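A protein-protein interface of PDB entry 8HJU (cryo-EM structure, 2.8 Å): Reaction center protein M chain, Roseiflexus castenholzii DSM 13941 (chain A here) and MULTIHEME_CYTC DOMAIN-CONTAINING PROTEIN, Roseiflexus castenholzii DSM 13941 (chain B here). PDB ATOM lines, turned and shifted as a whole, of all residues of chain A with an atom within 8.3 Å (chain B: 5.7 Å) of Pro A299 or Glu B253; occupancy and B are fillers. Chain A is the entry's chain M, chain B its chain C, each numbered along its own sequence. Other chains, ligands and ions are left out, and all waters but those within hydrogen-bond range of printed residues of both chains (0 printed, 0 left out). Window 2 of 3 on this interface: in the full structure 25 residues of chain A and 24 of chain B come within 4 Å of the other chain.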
ATOM      1  N   TYR A 284      21.741  17.718 -13.126  1.00  0.00           N
ATOM      2  CA  TYR A 284      22.199  16.338 -13.063  1.00  0.00           C
ATOM      3  C   TYR A 284      21.618  15.519 -14.206  1.00  0.00           C
ATOM      4  O   TYR A 284      22.330  14.729 -14.833  1.00  0.00           O
ATOM      5  CB  TYR A 284      21.837  15.719 -11.718  1.00  0.00           C
ATOM      6  CG  TYR A 284      22.165  14.252 -11.616  1.00  0.00           C
ATOM      7  CD1 TYR A 284      21.254  13.291 -12.015  1.00  0.00           C
ATOM      8  CD2 TYR A 284      23.379  13.829 -11.115  1.00  0.00           C
ATOM      9  CE1 TYR A 284      21.544  11.964 -11.922  1.00  0.00           C
ATOM     10  CE2 TYR A 284      23.675  12.497 -11.022  1.00  0.00           C
ATOM     11  CZ  TYR A 284      22.752  11.568 -11.428  1.00  0.00           C
ATOM     12  OH  TYR A 284      23.029  10.228 -11.340  1.00  0.00           O
ATOM     13  N   GLU A 288      23.786  13.664 -17.221  1.00  0.00           N
ATOM     14  CA  GLU A 288      23.754  12.280 -17.676  1.00  0.00           C
ATOM     15  C   GLU A 288      23.666  12.203 -19.192  1.00  0.00           C
ATOM     16  O   GLU A 288      24.303  11.350 -19.816  1.00  0.00           O
ATOM     17  CB  GLU A 288      22.584  11.544 -17.041  1.00  0.00           C
ATOM     18  CG  GLU A 288      22.685  11.391 -15.547  1.00  0.00           C
ATOM     19  CD  GLU A 288      21.474  10.697 -14.968  1.00  0.00           C
ATOM     20  OE1 GLU A 288      21.640   9.623 -14.355  1.00  0.00           O
ATOM     21  OE2 GLU A 288      20.357  11.227 -15.127  1.00  0.00           O
ATOM     22  N   ALA A 294      29.588  10.611 -13.497  1.00  0.00           N
ATOM     23  CA  ALA A 294      30.219   9.315 -13.305  1.00  0.00           C
ATOM     24  C   ALA A 294      29.176   8.282 -12.897  1.00  0.00           C
ATOM     25  O   ALA A 294      28.341   8.563 -12.031  1.00  0.00           O
ATOM     26  CB  ALA A 294      31.310   9.405 -12.248  1.00  0.00           C
ATOM     27  N   PRO A 295      29.180   7.094 -13.494  1.00  0.00           N
ATOM     28  CA  PRO A 295      28.287   6.036 -13.021  1.00  0.00           C
ATOM     29  C   PRO A 295      28.654   5.617 -11.612  1.00  0.00           C
ATOM     30  O   PRO A 295      29.830   5.487 -11.269  1.00  0.00           O
ATOM     31  CB  PRO A 295      28.518   4.898 -14.020  1.00  0.00           C
ATOM     32  CG  PRO A 295      29.146   5.542 -15.197  1.00  0.00           C
ATOM     33  CD  PRO A 295      29.950   6.672 -14.671  1.00  0.00           C
ATOM     34  N   TRP A 296      27.634   5.407 -10.792  1.00  0.00           N
ATOM     35  CA  TRP A 296      27.807   5.046  -9.388  1.00  0.00           C
ATOM     36  C   TRP A 296      26.870   3.890  -9.073  1.00  0.00           C
ATOM     37  O   TRP A 296      25.888   4.049  -8.338  1.00  0.00           O
ATOM     38  CB  TRP A 296      27.535   6.251  -8.491  1.00  0.00           C
ATOM     39  CG  TRP A 296      28.326   6.280  -7.241  1.00  0.00           C
ATOM     40  CD1 TRP A 296      29.168   5.321  -6.782  1.00  0.00           C
ATOM     41  CD2 TRP A 296      28.339   7.325  -6.267  1.00  0.00           C
ATOM     42  NE1 TRP A 296      29.713   5.703  -5.585  1.00  0.00           N
ATOM     43  CE2 TRP A 296      29.217   6.932  -5.248  1.00  0.00           C
ATOM     44  CE3 TRP A 296      27.694   8.558  -6.163  1.00  0.00           C
ATOM     45  CZ2 TRP A 296      29.465   7.725  -4.138  1.00  0.00           C
ATOM     46  CZ3 TRP A 296      27.946   9.340  -5.065  1.00  0.00           C
ATOM     47  CH2 TRP A 296      28.821   8.923  -4.066  1.00  0.00           C
ATOM     48  N   PRO A 297      27.150   2.703  -9.613  1.00  0.00           N
ATOM     49  CA  PRO A 297      26.210   1.585  -9.477  1.00  0.00           C
ATOM     50  C   PRO A 297      26.045   1.114  -8.044  1.00  0.00           C
ATOM     51  O   PRO A 297      24.920   0.989  -7.553  1.00  0.00           O
ATOM     52  CB  PRO A 297      26.837   0.489 -10.349  1.00  0.00           C
ATOM     53  CG  PRO A 297      27.858   1.173 -11.181  1.00  0.00           C
ATOM     54  CD  PRO A 297      28.348   2.314 -10.370  1.00  0.00           C
ATOM     55  N   ASN A 298      27.156   0.850  -7.361  1.00  0.00           N
ATOM     56  CA  ASN A 298      27.147   0.322  -5.998  1.00  0.00           C
ATOM     57  C   ASN A 298      27.969   1.232  -5.100  1.00  0.00           C
ATOM     58  O   ASN A 298      29.119   0.921  -4.765  1.00  0.00           O
ATOM     59  CB  ASN A 298      27.684  -1.107  -5.956  1.00  0.00           C
ATOM     60  CG  ASN A 298      27.091  -1.978  -7.034  1.00  0.00           C
ATOM     61  OD1 ASN A 298      27.599  -2.032  -8.152  1.00  0.00           O
ATOM     62  ND2 ASN A 298      26.003  -2.663  -6.706  1.00  0.00           N
ATOM     63  N   PRO A 299      27.412   2.362  -4.684  1.00  0.00           N
ATOM     64  CA  PRO A 299      28.143   3.242  -3.775  1.00  0.00           C
ATOM     65  C   PRO A 299      28.254   2.640  -2.387  1.00  0.00           C
ATOM     66  O   PRO A 299      27.385   1.893  -1.933  1.00  0.00           O
ATOM     67  CB  PRO A 299      27.299   4.518  -3.761  1.00  0.00           C
ATOM     68  CG  PRO A 299      25.959   4.098  -4.191  1.00  0.00           C
ATOM     69  CD  PRO A 299      26.122   2.934  -5.098  1.00  0.00           C
ATOM     70  N   ASP A 300      29.352   2.967  -1.713  1.00  0.00           N
ATOM     71  CA  ASP A 300      29.548   2.577  -0.321  1.00  0.00           C
ATOM     72  C   ASP A 300      28.903   3.642   0.547  1.00  0.00           C
ATOM     73  O   ASP A 300      29.495   4.690   0.804  1.00  0.00           O
ATOM     74  CB  ASP A 300      31.025   2.426   0.009  1.00  0.00           C
ATOM     75  CG  ASP A 300      31.256   2.158   1.477  1.00  0.00           C
ATOM     76  OD1 ASP A 300      30.751   1.131   1.975  1.00  0.00           O
ATOM     77  OD2 ASP A 300      31.926   2.977   2.138  1.00  0.00           O
ATOM     78  N   TRP A 301      27.723   3.323   1.046  1.00  0.00           N
ATOM     79  CA  TRP A 301      27.003   4.318   1.755  1.00  0.00           C
ATOM     80  C   TRP A 301      27.199   4.319   3.216  1.00  0.00           C
ATOM     81  O   TRP A 301      26.557   5.075   3.904  1.00  0.00           O
ATOM     82  CB  TRP A 301      25.564   4.218   1.372  1.00  0.00           C
ATOM     83  CG  TRP A 301      24.968   5.545   1.139  1.00  0.00           C
ATOM     84  CD1 TRP A 301      24.009   6.139   1.876  1.00  0.00           C
ATOM     85  CD2 TRP A 301      25.317   6.469   0.110  1.00  0.00           C
ATOM     86  NE1 TRP A 301      23.728   7.366   1.372  1.00  0.00           N
ATOM     87  CE2 TRP A 301      24.516   7.596   0.283  1.00  0.00           C
ATOM     88  CE3 TRP A 301      26.224   6.447  -0.945  1.00  0.00           C
ATOM     89  CZ2 TRP A 301      24.599   8.696  -0.546  1.00  0.00           C
ATOM     90  CZ3 TRP A 301      26.295   7.531  -1.769  1.00  0.00           C
ATOM     91  CH2 TRP A 301      25.490   8.640  -1.568  1.00  0.00           C
ATOM     92  N   ALA A 302      28.067   3.471   3.700  1.00  0.00           N
ATOM     93  CA  ALA A 302      28.388   3.473   5.119  1.00  0.00           C
ATOM     94  C   ALA A 302      29.084   4.760   5.523  1.00  0.00           C
ATOM     95  O   ALA A 302      29.025   5.157   6.690  1.00  0.00           O
ATOM     96  CB  ALA A 302      29.257   2.268   5.464  1.00  0.00           C
ATOM     97  N   GLN A 303      29.743   5.424   4.575  1.00  0.00           N
ATOM     98  CA  GLN A 303      30.426   6.674   4.880  1.00  0.00           C
ATOM     99  C   GLN A 303      29.437   7.775   5.222  1.00  0.00           C
ATOM    100  O   GLN A 303      29.710   8.618   6.082  1.00  0.00           O
ATOM    101  CB  GLN A 303      31.293   7.096   3.697  1.00  0.00           C
ATOM    102  CG  GLN A 303      31.948   8.442   3.875  1.00  0.00           C
ATOM    103  CD  GLN A 303      32.568   8.962   2.606  1.00  0.00           C
ATOM    104  OE1 GLN A 303      33.141  10.044   2.585  1.00  0.00           O
ATOM    105  NE2 GLN A 303      32.460   8.193   1.539  1.00  0.00           N
ATOM    106  N   TYR A 304      28.282   7.774   4.570  1.00  0.00           N
ATOM    107  CA  TYR A 304      27.347   8.881   4.634  1.00  0.00           C
ATOM    108  C   TYR A 304      26.237   8.670   5.645  1.00  0.00           C
ATOM    109  O   TYR A 304      25.336   9.505   5.737  1.00  0.00           O
ATOM    110  CB  TYR A 304      26.749   9.121   3.252  1.00  0.00           C
ATOM    111  CG  TYR A 304      27.792   9.411   2.214  1.00  0.00           C
ATOM    112  CD1 TYR A 304      28.580  10.543   2.301  1.00  0.00           C
ATOM    113  CD2 TYR A 304      28.003   8.549   1.158  1.00  0.00           C
ATOM    114  CE1 TYR A 304      29.540  10.813   1.358  1.00  0.00           C
ATOM    115  CE2 TYR A 304      28.959   8.814   0.209  1.00  0.00           C
ATOM    116  CZ  TYR A 304      29.722   9.949   0.312  1.00  0.00           C
ATOM    117  OH  TYR A 304      30.680  10.217  -0.629  1.00  0.00           O
ATOM    118  N   ASN B 245      20.942  10.217  -2.277  1.00  0.00           N
ATOM    119  CA  ASN B 245      22.240  10.483  -2.875  1.00  0.00           C
ATOM    120  C   ASN B 245      22.222  11.963  -3.222  1.00  0.00           C
ATOM    121  O   ASN B 245      21.573  12.377  -4.180  1.00  0.00           O
ATOM    122  CB  ASN B 245      22.480   9.608  -4.097  1.00  0.00           C
ATOM    123  CG  ASN B 245      23.908   9.660  -4.574  1.00  0.00           C
ATOM    124  OD1 ASN B 245      24.577  10.671  -4.434  1.00  0.00           O
ATOM    125  ND2 ASN B 245      24.385   8.566  -5.131  1.00  0.00           N
ATOM    126  N   ARG B 247      23.834  13.973  -4.772  1.00  0.00           N
ATOM    127  CA  ARG B 247      24.100  14.440  -6.125  1.00  0.00           C
ATOM    128  C   ARG B 247      22.826  14.495  -6.956  1.00  0.00           C
ATOM    129  O   ARG B 247      22.747  15.269  -7.913  1.00  0.00           O
ATOM    130  CB  ARG B 247      25.158  13.563  -6.790  1.00  0.00           C
ATOM    131  CG  ARG B 247      24.656  12.311  -7.460  1.00  0.00           C
ATOM    132  CD  ARG B 247      25.805  11.576  -8.113  1.00  0.00           C
ATOM    133  NE  ARG B 247      25.360  10.413  -8.865  1.00  0.00           N
ATOM    134  CZ  ARG B 247      26.113   9.745  -9.728  1.00  0.00           C
ATOM    135  NH1 ARG B 247      27.359  10.124  -9.957  1.00  0.00           N
ATOM    136  NH2 ARG B 247      25.619   8.699 -10.362  1.00  0.00           N
ATOM    137  N   SER B 251      16.482  10.969  -6.954  1.00  0.00           N
ATOM    138  CA  SER B 251      16.803   9.563  -7.136  1.00  0.00           C
ATOM    139  C   SER B 251      16.381   8.749  -5.925  1.00  0.00           C
ATOM    140  O   SER B 251      16.461   9.212  -4.786  1.00  0.00           O
ATOM    141  CB  SER B 251      18.297   9.393  -7.386  1.00  0.00           C
ATOM    142  OG  SER B 251      18.632   8.029  -7.520  1.00  0.00           O
ATOM    143  N   TYR B 252      15.941   7.519  -6.178  1.00  0.00           N
ATOM    144  CA  TYR B 252      15.549   6.571  -5.137  1.00  0.00           C
ATOM    145  C   TYR B 252      16.628   5.524  -4.908  1.00  0.00           C
ATOM    146  O   TYR B 252      16.349   4.340  -4.721  1.00  0.00           O
ATOM    147  CB  TYR B 252      14.218   5.922  -5.489  1.00  0.00           C
ATOM    148  CG  TYR B 252      13.032   6.779  -5.137  1.00  0.00           C
ATOM    149  CD1 TYR B 252      12.570   7.744  -6.007  1.00  0.00           C
ATOM    150  CD2 TYR B 252      12.383   6.633  -3.926  1.00  0.00           C
ATOM    151  CE1 TYR B 252      11.494   8.529  -5.686  1.00  0.00           C
ATOM    152  CE2 TYR B 252      11.306   7.416  -3.596  1.00  0.00           C
ATOM    153  CZ  TYR B 252      10.866   8.363  -4.480  1.00  0.00           C
ATOM    154  OH  TYR B 252       9.790   9.148  -4.157  1.00  0.00           O
ATOM    155  N   GLU B 253      17.881   5.971  -4.938  1.00  0.00           N
ATOM    156  CA  GLU B 253      19.029   5.083  -4.797  1.00  0.00           C
ATOM    157  C   GLU B 253      19.019   4.345  -3.466  1.00  0.00           C
ATOM    158  O   GLU B 253      19.246   3.133  -3.414  1.00  0.00           O
ATOM    159  CB  GLU B 253      20.313   5.899  -4.920  1.00  0.00           C
ATOM    160  CG  GLU B 253      21.013   5.820  -6.244  1.00  0.00           C
ATOM    161  CD  GLU B 253      22.469   6.215  -6.127  1.00  0.00           C
ATOM    162  OE1 GLU B 253      23.090   5.876  -5.099  1.00  0.00           O
ATOM    163  OE2 GLU B 253      22.990   6.870  -7.053  1.00  0.00           O
ATOM    164  N   ILE B 254      18.772   5.067  -2.372  1.00  0.00           N
ATOM    165  CA  ILE B 254      19.176   4.583  -1.057  1.00  0.00           C
ATOM    166  C   ILE B 254      18.167   3.629  -0.429  1.00  0.00           C
ATOM    167  O   ILE B 254      18.526   2.895   0.499  1.00  0.00           O
ATOM    168  CB  ILE B 254      19.461   5.788  -0.147  1.00  0.00           C
ATOM    169  CG1 ILE B 254      20.381   6.764  -0.865  1.00  0.00           C
ATOM    170  CG2 ILE B 254      20.133   5.366   1.129  1.00  0.00           C
ATOM    171  CD1 ILE B 254      21.676   6.153  -1.306  1.00  0.00           C
ATOM    172  N   ALA B 255      16.923   3.621  -0.901  1.00  0.00           N
ATOM    173  CA  ALA B 255      15.894   2.667  -0.484  1.00  0.00           C
ATOM    174  C   ALA B 255      15.371   2.951   0.916  1.00  0.00           C
ATOM    175  O   ALA B 255      14.386   2.346   1.340  1.00  0.00           O
ATOM    176  CB  ALA B 255      16.402   1.226  -0.562  1.00  0.00           C
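Pro A299 touches one residue of chain B.
Of the printed residues of chain A, Arg B247 touches Tyr A284, Ala A294 and Trp A296.
Printed residues of chain B within 4 Å of Tyr A284: Arg B247.
Of the printed residues of chain A, Ile B254 touches Trp A301 (3.6 Å).
Printed residues of chain A within 4 Å of Asn B245: Trp A296 and Trp A301.
Pro A295 touches none of the printed residues of chain B.
The nearest residue of chain B that does not touch Pro A299 is Asn B245 (4.8 Å).
The nearest residue of chain A that does not touch Glu B253 is Trp A296 (4.2 Å).
The nearest printed residue of chain B that does not touch Ala A294 is Glu B253 (7.5 Å).
O of Ala A294 lies within hydrogen-bond range of NH1 of Arg B247 (2.8 Å).
NH2 of Arg B247 lies within hydrogen-bond range of OH of Tyr A284, at 3.2 Å.
Hydrophobic or aromatic side chains of chain A that line the printed part of chain B: Tyr A284, Trp A296, Pro A299 and Trp A301.
Along chain A the printed residues that touch a printed residue of chain B span positions 284 to 301.
Hydrophobic or aromatic side chains of chain B within 4 Å of the printed part of chain A: Ile B254.
ND2 of Asn B245 touches CE3 of Trp A296, at 3.5 Å.
Arg B247 touches Trp A296.
Glu B253 touches Pro A299 (OE1 to CG, 3.5 Å).
CG of Asn B245 touches CH2 of Trp A301, 3.5 Å away.
Trp A301 touches Ile B254.
The side-chain amide oxygen (OD1) of Asn B245 sits close to the backbone NH (N) of Arg B247 (3.4 Å).
N of Glu B253 sits close to OG of Ser B251 (3.4 Å).
ND2 of Asn B245 is in hydrogen-bond range of OE2 of Glu B253, 2.9 Å away.
The side-chain hydroxyl (OH) of Tyr A284 lies within hydrogen-bond range of the side-chain carboxylate (OE1) of Glu A288.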
